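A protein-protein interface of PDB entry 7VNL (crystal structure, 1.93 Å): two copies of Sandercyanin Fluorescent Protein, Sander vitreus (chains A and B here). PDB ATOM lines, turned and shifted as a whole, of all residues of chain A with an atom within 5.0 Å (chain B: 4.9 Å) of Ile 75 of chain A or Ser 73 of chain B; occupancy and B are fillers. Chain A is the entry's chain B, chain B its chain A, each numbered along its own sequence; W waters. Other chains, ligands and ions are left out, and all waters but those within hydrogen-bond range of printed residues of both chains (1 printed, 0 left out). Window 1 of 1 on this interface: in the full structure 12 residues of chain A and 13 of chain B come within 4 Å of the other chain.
The backbone carbonyl oxygen (O) of Ile 75 of chain B sits at hydrogen-bond distance from the backbone NH (N) of Gln 86 of chain B.
N of Phe 88 of chain A lies within hydrogen-bond range of O of Ser 73 of chain A, 2.8 Å away.
N of Gln 86 of chain A is in hydrogen-bond range of O of Ile 75 of chain A (2.7 Å).
OG of Ser 49 of chain A sits at hydrogen-bond distance from N of Gly 51 of chain A (3.1 Å).
OG of Ser 49 of chain A is in hydrogen-bond range of O of Val 52 of chain A (3.5 Å).
The backbone NH (N) of Val 56 of chain B lies within hydrogen-bond range of the backbone carbonyl oxygen (O) of Gly 72 of chain B, at 2.9 Å.
Ile 75 of chain A touches three residues of chain B.
Ser 73 of chain B touches just these residues of chain A: Gly 51, Val 52 and Ile 75.
Printed residues of chain B within 4 Å of Phe 88 of chain A: Ile 75 (3.5 Å) and Phe 88 (3.7 Å).
Of the printed residues of chain A, Phe 88 of chain B touches Val 52, Ile 75, Glu 77 and Phe 88.
Printed residues of chain B within 4 Å of Gly 51 of chain A: Ser 55 (3.9 Å), Ile 71 (3.9 Å), Gly 72 (3.2 Å) and Ser 73 (3.4 Å).
Gln 86 of chain A touches none of the printed residues of chain B.
Gln 86 of chain B touches none of the printed residues of chain A.
Ser 73 of chain A touches Ile 75 of chain B, and with the chains exchanged Ile 75 of chain A touches Ser 73 of chain B.
Ile 75 of chain B touches its own counterpart, Ile 75 of chain A.
Ile 75 of chain A touches Phe 88 of chain B, and with the chains exchanged Phe 88 of chain A touches Ile 75 of chain B.
Phe 88 of chain B touches its own counterpart, Phe 88 of chain A.
5 positions are printed for both chains.
Of the 15 pairs that touch across the chains among the printed residues, 6 have their exchanged pair printed and touching as well.
Water W1 lies within hydrogen-bond range of the side-chain hydroxyl (OG) of Ser 73 of chain B (3.1 Å) and the side-chain hydroxyl (OG) of Ser 49 of chain A (3.4 Å).
Among the printed residues, pairs that only touch across the chains: Gly 51 of chain A with Gly 72 of chain B, Glu 77 of chain A with Phe 88 of chain B, Gly 51 of chain A with Ser 73 of chain B, Val 52 of chain A with Phe 88 of chain B, Phe 88 of chain A with Ile 75 of chain B, Ile 75 of chain A with Phe 88 of chain B, Phe 88 of chain A with Phe 88 of chain B, Ile 75 of chain A with Ile 75 of chain B, Gly 51 of chain A with Ile 71 of chain B, Ile 75 of chain A with Ser 73 of chain B, Val 52 of chain A with Ile 71 of chain B, Val 52 of chain A with Gly 72 of chain B, Gly 51 of chain A with Ser 55 of chain B and Ser 73 of chain A with Ile 75 of chain B.
The side-chain hydroxyl (OG) of Ser 73 of chain B is in hydrogen-bond range of the backbone NH (N) of Val 52 of chain A (3.0 Å).
Of the 13 printed residues of chain A, 6 touch a printed residue of chain B.
Hydrophobic or aromatic side chains of chain A that line the printed part of chain B: Val 52, Ile 75 and Phe 88.
Printed residues of chain B that touch a printed residue of chain A: Ser 55, Ile 71, Gly 72, Ser 73, Ile 75 and Phe 88.
Hydrophobic or aromatic side chains of chain B within 4 Å of the printed part of chain A: Ile 71, Ile 75 and Phe 88.
Among the printed residues, 15 pairs touch across the chains.
Among the printed residues, no Asp or Glu carboxylate lies within 4 Å of a Lys or Arg side-chain nitrogen of the other chain.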
ATOM      1  N   SER A  49     -19.493  16.415   3.176  1.00  0.00           N
ATOM      2  CA  SER A  49     -19.569  15.878   1.835  1.00  0.00           C
ATOM      3  C   SER A  49     -20.092  14.449   1.893  1.00  0.00           C
ATOM      4  O   SER A  49     -19.700  13.690   2.786  1.00  0.00           O
ATOM      5  CB  SER A  49     -18.183  15.907   1.173  1.00  0.00           C
ATOM      6  OG  SER A  49     -18.088  15.018   0.072  1.00  0.00           O
ATOM      7  N   GLY A  51     -19.344  12.202  -0.189  1.00  0.00           N
ATOM      8  CA  GLY A  51     -18.158  11.425  -0.496  1.00  0.00           C
ATOM      9  C   GLY A  51     -17.123  11.540   0.601  1.00  0.00           C
ATOM     10  O   GLY A  51     -17.447  11.716   1.780  1.00  0.00           O
ATOM     11  N   VAL A  52     -15.859  11.445   0.217  1.00  0.00           N
ATOM     12  CA  VAL A  52     -14.771  11.677   1.153  1.00  0.00           C
ATOM     13  C   VAL A  52     -14.462  13.169   1.194  1.00  0.00           C
ATOM     14  O   VAL A  52     -14.818  13.933   0.293  1.00  0.00           O
ATOM     15  CB  VAL A  52     -13.518  10.844   0.793  1.00  0.00           C
ATOM     16  CG1 VAL A  52     -13.891   9.389   0.603  1.00  0.00           C
ATOM     17  CG2 VAL A  52     -12.887  11.375  -0.464  1.00  0.00           C
ATOM     18  N   GLY A  53     -13.793  13.595   2.259  1.00  0.00           N
ATOM     19  CA  GLY A  53     -13.375  14.982   2.348  1.00  0.00           C
ATOM     20  C   GLY A  53     -14.531  15.878   2.751  1.00  0.00           C
ATOM     21  O   GLY A  53     -15.519  15.438   3.343  1.00  0.00           O
ATOM     22  N   SER A  73     -14.011  21.290  -3.606  1.00  0.00           N
ATOM     23  CA  SER A  73     -13.973  20.074  -2.806  1.00  0.00           C
ATOM     24  C   SER A  73     -12.593  19.944  -2.189  1.00  0.00           C
ATOM     25  O   SER A  73     -11.595  20.256  -2.840  1.00  0.00           O
ATOM     26  CB  SER A  73     -14.284  18.827  -3.654  1.00  0.00           C
ATOM     27  OG  SER A  73     -15.619  18.838  -4.107  1.00  0.00           O
ATOM     28  N   ALA A  74     -12.541  19.471  -0.943  1.00  0.00           N
ATOM     29  CA  ALA A  74     -11.291  19.260  -0.221  1.00  0.00           C
ATOM     30  C   ALA A  74     -11.137  17.782   0.085  1.00  0.00           C
ATOM     31  O   ALA A  74     -12.071  17.164   0.600  1.00  0.00           O
ATOM     32  CB  ALA A  74     -11.273  20.042   1.092  1.00  0.00           C
ATOM     33  N   ILE A  75      -9.968  17.218  -0.217  1.00  0.00           N
ATOM     34  CA  ILE A  75      -9.735  15.788  -0.009  1.00  0.00           C
ATOM     35  C   ILE A  75      -8.334  15.581   0.549  1.00  0.00           C
ATOM     36  O   ILE A  75      -7.377  16.221   0.100  1.00  0.00           O
ATOM     37  CB  ILE A  75      -9.922  14.996  -1.324  1.00  0.00           C
ATOM     38  CG1 ILE A  75     -11.376  15.110  -1.808  1.00  0.00           C
ATOM     39  CG2 ILE A  75      -9.537  13.518  -1.120  1.00  0.00           C
ATOM     40  CD1 ILE A  75     -11.660  14.354  -3.060  1.00  0.00           C
ATOM     41  N   ALA A  76      -8.215  14.692   1.535  1.00  0.00           N
ATOM     42  CA  ALA A  76      -6.912  14.211   1.992  1.00  0.00           C
ATOM     43  C   ALA A  76      -6.547  13.001   1.147  1.00  0.00           C
ATOM     44  O   ALA A  76      -7.049  11.899   1.387  1.00  0.00           O
ATOM     45  CB  ALA A  76      -6.942  13.848   3.474  1.00  0.00           C
ATOM     46  N   GLU A  77      -5.659  13.197   0.163  1.00  0.00           N
ATOM     47  CA  GLU A  77      -5.329  12.105  -0.756  1.00  0.00           C
ATOM     48  C   GLU A  77      -4.647  10.945  -0.038  1.00  0.00           C
ATOM     49  O   GLU A  77      -4.813   9.787  -0.441  1.00  0.00           O
ATOM     50  CB  GLU A  77      -4.429  12.612  -1.876  1.00  0.00           C
ATOM     51  CG  GLU A  77      -5.026  13.808  -2.602  1.00  0.00           C
ATOM     52  CD  GLU A  77      -4.429  14.054  -3.976  1.00  0.00           C
ATOM     53  OE1 GLU A  77      -5.179  14.469  -4.883  1.00  0.00           O
ATOM     54  OE2 GLU A  77      -3.228  13.789  -4.164  1.00  0.00           O
ATOM     55  N   LYS A  84      -3.072  17.239   5.399  1.00  0.00           N
ATOM     56  CA  LYS A  84      -2.500  17.618   4.109  1.00  0.00           C
ATOM     57  C   LYS A  84      -3.574  17.365   3.060  1.00  0.00           C
ATOM     58  O   LYS A  84      -3.727  16.257   2.536  1.00  0.00           O
ATOM     59  CB  LYS A  84      -1.222  16.847   3.804  1.00  0.00           C
ATOM     60  CG  LYS A  84      -0.042  17.287   4.661  1.00  0.00           C
ATOM     61  CD  LYS A  84       1.213  16.526   4.301  1.00  0.00           C
ATOM     62  CE  LYS A  84       2.340  16.921   5.240  1.00  0.00           C
ATOM     63  NZ  LYS A  84       3.674  16.462   4.769  1.00  0.00           N
ATOM     64  N   LEU A  85      -4.316  18.406   2.749  1.00  0.00           N
ATOM     65  CA  LEU A  85      -5.442  18.276   1.852  1.00  0.00           C
ATOM     66  C   LEU A  85      -5.061  18.741   0.456  1.00  0.00           C
ATOM     67  O   LEU A  85      -4.061  19.435   0.245  1.00  0.00           O
ATOM     68  CB  LEU A  85      -6.629  19.089   2.380  1.00  0.00           C
ATOM     69  CG  LEU A  85      -7.040  18.604   3.784  1.00  0.00           C
ATOM     70  CD1 LEU A  85      -7.417  19.763   4.666  1.00  0.00           C
ATOM     71  CD2 LEU A  85      -8.197  17.654   3.677  1.00  0.00           C
ATOM     72  N   GLN A  86      -5.892  18.356  -0.495  1.00  0.00           N
ATOM     73  CA  GLN A  86      -5.868  18.887  -1.843  1.00  0.00           C
ATOM     74  C   GLN A  86      -7.212  19.556  -2.082  1.00  0.00           C
ATOM     75  O   GLN A  86      -8.260  18.962  -1.802  1.00  0.00           O
ATOM     76  CB  GLN A  86      -5.605  17.764  -2.852  1.00  0.00           C
ATOM     77  CG  GLN A  86      -5.023  18.226  -4.164  1.00  0.00           C
ATOM     78  CD  GLN A  86      -3.527  18.457  -4.100  1.00  0.00           C
ATOM     79  OE1 GLN A  86      -2.875  18.171  -3.092  1.00  0.00           O
ATOM     80  NE2 GLN A  86      -2.973  18.960  -5.184  1.00  0.00           N
ATOM     81  N   PHE A  88      -9.829  21.299  -4.715  1.00  0.00           N
ATOM     82  CA  PHE A  88     -10.253  21.299  -6.110  1.00  0.00           C
ATOM     83  C   PHE A  88     -11.343  22.358  -6.248  1.00  0.00           C
ATOM     84  O   PHE A  88     -12.491  22.115  -5.881  1.00  0.00           O
ATOM     85  CB  PHE A  88     -10.759  19.907  -6.515  1.00  0.00           C
ATOM     86  CG  PHE A  88      -9.767  18.793  -6.250  1.00  0.00           C
ATOM     87  CD1 PHE A  88      -9.736  18.134  -5.025  1.00  0.00           C
ATOM     88  CD2 PHE A  88      -8.889  18.389  -7.246  1.00  0.00           C
ATOM     89  CE1 PHE A  88      -8.800  17.107  -4.779  1.00  0.00           C
ATOM     90  CE2 PHE A  88      -7.960  17.354  -7.017  1.00  0.00           C
ATOM     91  CZ  PHE A  88      -7.920  16.721  -5.789  1.00  0.00           C
ATOM     92  N   PHE B  54     -18.410  14.617  -8.390  1.00  0.00           N
ATOM     93  CA  PHE B  54     -19.610  13.960  -7.903  1.00  0.00           C
ATOM     94  C   PHE B  54     -19.219  12.930  -6.865  1.00  0.00           C
ATOM     95  O   PHE B  54     -18.041  12.604  -6.671  1.00  0.00           O
ATOM     96  CB  PHE B  54     -20.457  13.350  -9.050  1.00  0.00           C
ATOM     97  CG  PHE B  54     -19.708  12.372  -9.939  1.00  0.00           C
ATOM     98  CD1 PHE B  54     -19.678  11.025  -9.649  1.00  0.00           C
ATOM     99  CD2 PHE B  54     -19.088  12.813 -11.105  1.00  0.00           C
ATOM    100  CE1 PHE B  54     -19.000  10.131 -10.482  1.00  0.00           C
ATOM    101  CE2 PHE B  54     -18.425  11.929 -11.955  1.00  0.00           C
ATOM    102  CZ  PHE B  54     -18.379  10.590 -11.645  1.00  0.00           C
ATOM    103  N   SER B  55     -20.227  12.462  -6.157  1.00  0.00           N
ATOM    104  CA  SER B  55     -20.005  11.570  -5.043  1.00  0.00           C
ATOM    105  C   SER B  55     -20.302  10.138  -5.484  1.00  0.00           C
ATOM    106  O   SER B  55     -21.056   9.903  -6.433  1.00  0.00           O
ATOM    107  CB  SER B  55     -20.839  12.032  -3.841  1.00  0.00           C
ATOM    108  OG  SER B  55     -22.176  11.600  -3.926  1.00  0.00           O
ATOM    109  N   VAL B  56     -19.651   9.188  -4.811  1.00  0.00           N
ATOM    110  CA  VAL B  56     -19.605   7.787  -5.219  1.00  0.00           C
ATOM    111  C   VAL B  56     -20.114   6.932  -4.067  1.00  0.00           C
ATOM    112  O   VAL B  56     -19.723   7.143  -2.913  1.00  0.00           O
ATOM    113  CB  VAL B  56     -18.173   7.367  -5.607  1.00  0.00           C
ATOM    114  CG1 VAL B  56     -18.121   5.886  -5.939  1.00  0.00           C
ATOM    115  CG2 VAL B  56     -17.661   8.223  -6.798  1.00  0.00           C
ATOM    116  N   ILE B  71     -17.733   4.557   0.136  1.00  0.00           N
ATOM    117  CA  ILE B  71     -18.016   5.911  -0.314  1.00  0.00           C
ATOM    118  C   ILE B  71     -16.759   6.486  -0.939  1.00  0.00           C
ATOM    119  O   ILE B  71     -15.625   6.096  -0.609  1.00  0.00           O
ATOM    120  CB  ILE B  71     -18.529   6.801   0.834  1.00  0.00           C
ATOM    121  CG1 ILE B  71     -17.358   7.373   1.631  1.00  0.00           C
ATOM    122  CG2 ILE B  71     -19.449   5.985   1.728  1.00  0.00           C
ATOM    123  CD1 ILE B  71     -17.750   8.045   2.948  1.00  0.00           C
ATOM    124  N   GLY B  72     -16.961   7.403  -1.877  1.00  0.00           N
ATOM    125  CA  GLY B  72     -15.842   8.051  -2.525  1.00  0.00           C
ATOM    126  C   GLY B  72     -16.268   9.374  -3.121  1.00  0.00           C
ATOM    127  O   GLY B  72     -17.438   9.763  -3.075  1.00  0.00           O
ATOM    128  N   SER B  73     -15.290  10.061  -3.691  1.00  0.00           N
ATOM    129  CA  SER B  73     -15.516  11.274  -4.457  1.00  0.00           C
ATOM    130  C   SER B  73     -14.796  11.137  -5.786  1.00  0.00           C
ATOM    131  O   SER B  73     -13.687  10.591  -5.849  1.00  0.00           O
ATOM    132  CB  SER B  73     -15.011  12.512  -3.713  1.00  0.00           C
ATOM    133  OG  SER B  73     -15.689  12.642  -2.479  1.00  0.00           O
ATOM    134  N   ALA B  74     -15.435  11.638  -6.838  1.00  0.00           N
ATOM    135  CA  ALA B  74     -14.887  11.634  -8.187  1.00  0.00           C
ATOM    136  C   ALA B  74     -14.664  13.067  -8.624  1.00  0.00           C
ATOM    137  O   ALA B  74     -15.571  13.897  -8.506  1.00  0.00           O
ATOM    138  CB  ALA B  74     -15.843  10.957  -9.160  1.00  0.00           C
ATOM    139  N   ILE B  75     -13.466  13.360  -9.122  1.00  0.00           N
ATOM    140  CA  ILE B  75     -13.148  14.698  -9.597  1.00  0.00           C
ATOM    141  C   ILE B  75     -12.363  14.584 -10.887  1.00  0.00           C
ATOM    142  O   ILE B  75     -11.424  13.787 -10.985  1.00  0.00           O
ATOM    143  CB  ILE B  75     -12.348  15.511  -8.558  1.00  0.00           C
ATOM    144  CG1 ILE B  75     -13.206  15.718  -7.299  1.00  0.00           C
ATOM    145  CG2 ILE B  75     -11.911  16.877  -9.159  1.00  0.00           C
ATOM    146  CD1 ILE B  75     -12.481  16.348  -6.145  1.00  0.00           C
ATOM    147  N   GLN B  86     -10.387  11.308 -11.348  1.00  0.00           N
ATOM    148  CA  GLN B  86      -9.674  10.674 -10.253  1.00  0.00           C
ATOM    149  C   GLN B  86     -10.710  10.305  -9.207  1.00  0.00           C
ATOM    150  O   GLN B  86     -11.550  11.137  -8.854  1.00  0.00           O
ATOM    151  CB  GLN B  86      -8.613  11.601  -9.647  1.00  0.00           C
ATOM    152  CG  GLN B  86      -7.353  11.766 -10.484  1.00  0.00           C
ATOM    153  CD  GLN B  86      -6.490  10.502 -10.532  1.00  0.00           C
ATOM    154  OE1 GLN B  86      -6.159  10.006 -11.606  1.00  0.00           O
ATOM    155  NE2 GLN B  86      -6.097  10.005  -9.369  1.00  0.00           N
ATOM    156  N   PHE B  87     -10.650   9.071  -8.720  1.00  0.00           N
ATOM    157  CA  PHE B  87     -11.560   8.581  -7.691  1.00  0.00           C
ATOM    158  C   PHE B  87     -10.821   8.488  -6.370  1.00  0.00           C
ATOM    159  O   PHE B  87      -9.731   7.910  -6.301  1.00  0.00           O
ATOM    160  CB  PHE B  87     -12.155   7.210  -8.042  1.00  0.00           C
ATOM    161  CG  PHE B  87     -13.428   7.280  -8.849  1.00  0.00           C
ATOM    162  CD1 PHE B  87     -13.571   8.210  -9.876  1.00  0.00           C
ATOM    163  CD2 PHE B  87     -14.475   6.400  -8.589  1.00  0.00           C
ATOM    164  CE1 PHE B  87     -14.745   8.253 -10.643  1.00  0.00           C
ATOM    165  CE2 PHE B  87     -15.662   6.449  -9.331  1.00  0.00           C
ATOM    166  CZ  PHE B  87     -15.797   7.375 -10.359  1.00  0.00           C
ATOM    167  N   PHE B  88     -11.430   9.042  -5.328  1.00  0.00           N
ATOM    168  CA  PHE B  88     -10.864   9.072  -3.983  1.00  0.00           C
ATOM    169  C   PHE B  88     -11.832   8.288  -3.109  1.00  0.00           C
ATOM    170  O   PHE B  88     -12.897   8.798  -2.764  1.00  0.00           O
ATOM    171  CB  PHE B  88     -10.714  10.510  -3.491  1.00  0.00           C
ATOM    172  CG  PHE B  88      -9.926  11.392  -4.422  1.00  0.00           C
ATOM    173  CD1 PHE B  88     -10.558  12.075  -5.454  1.00  0.00           C
ATOM    174  CD2 PHE B  88      -8.552  11.521  -4.281  1.00  0.00           C
ATOM    175  CE1 PHE B  88      -9.820  12.901  -6.318  1.00  0.00           C
ATOM    176  CE2 PHE B  88      -7.813  12.348  -5.132  1.00  0.00           C
ATOM    177  CZ  PHE B  88      -8.464  13.038  -6.158  1.00  0.00           C
HETATM  178  O   HOH W   1     -18.266  14.100  -3.229  1.00  0.00           O
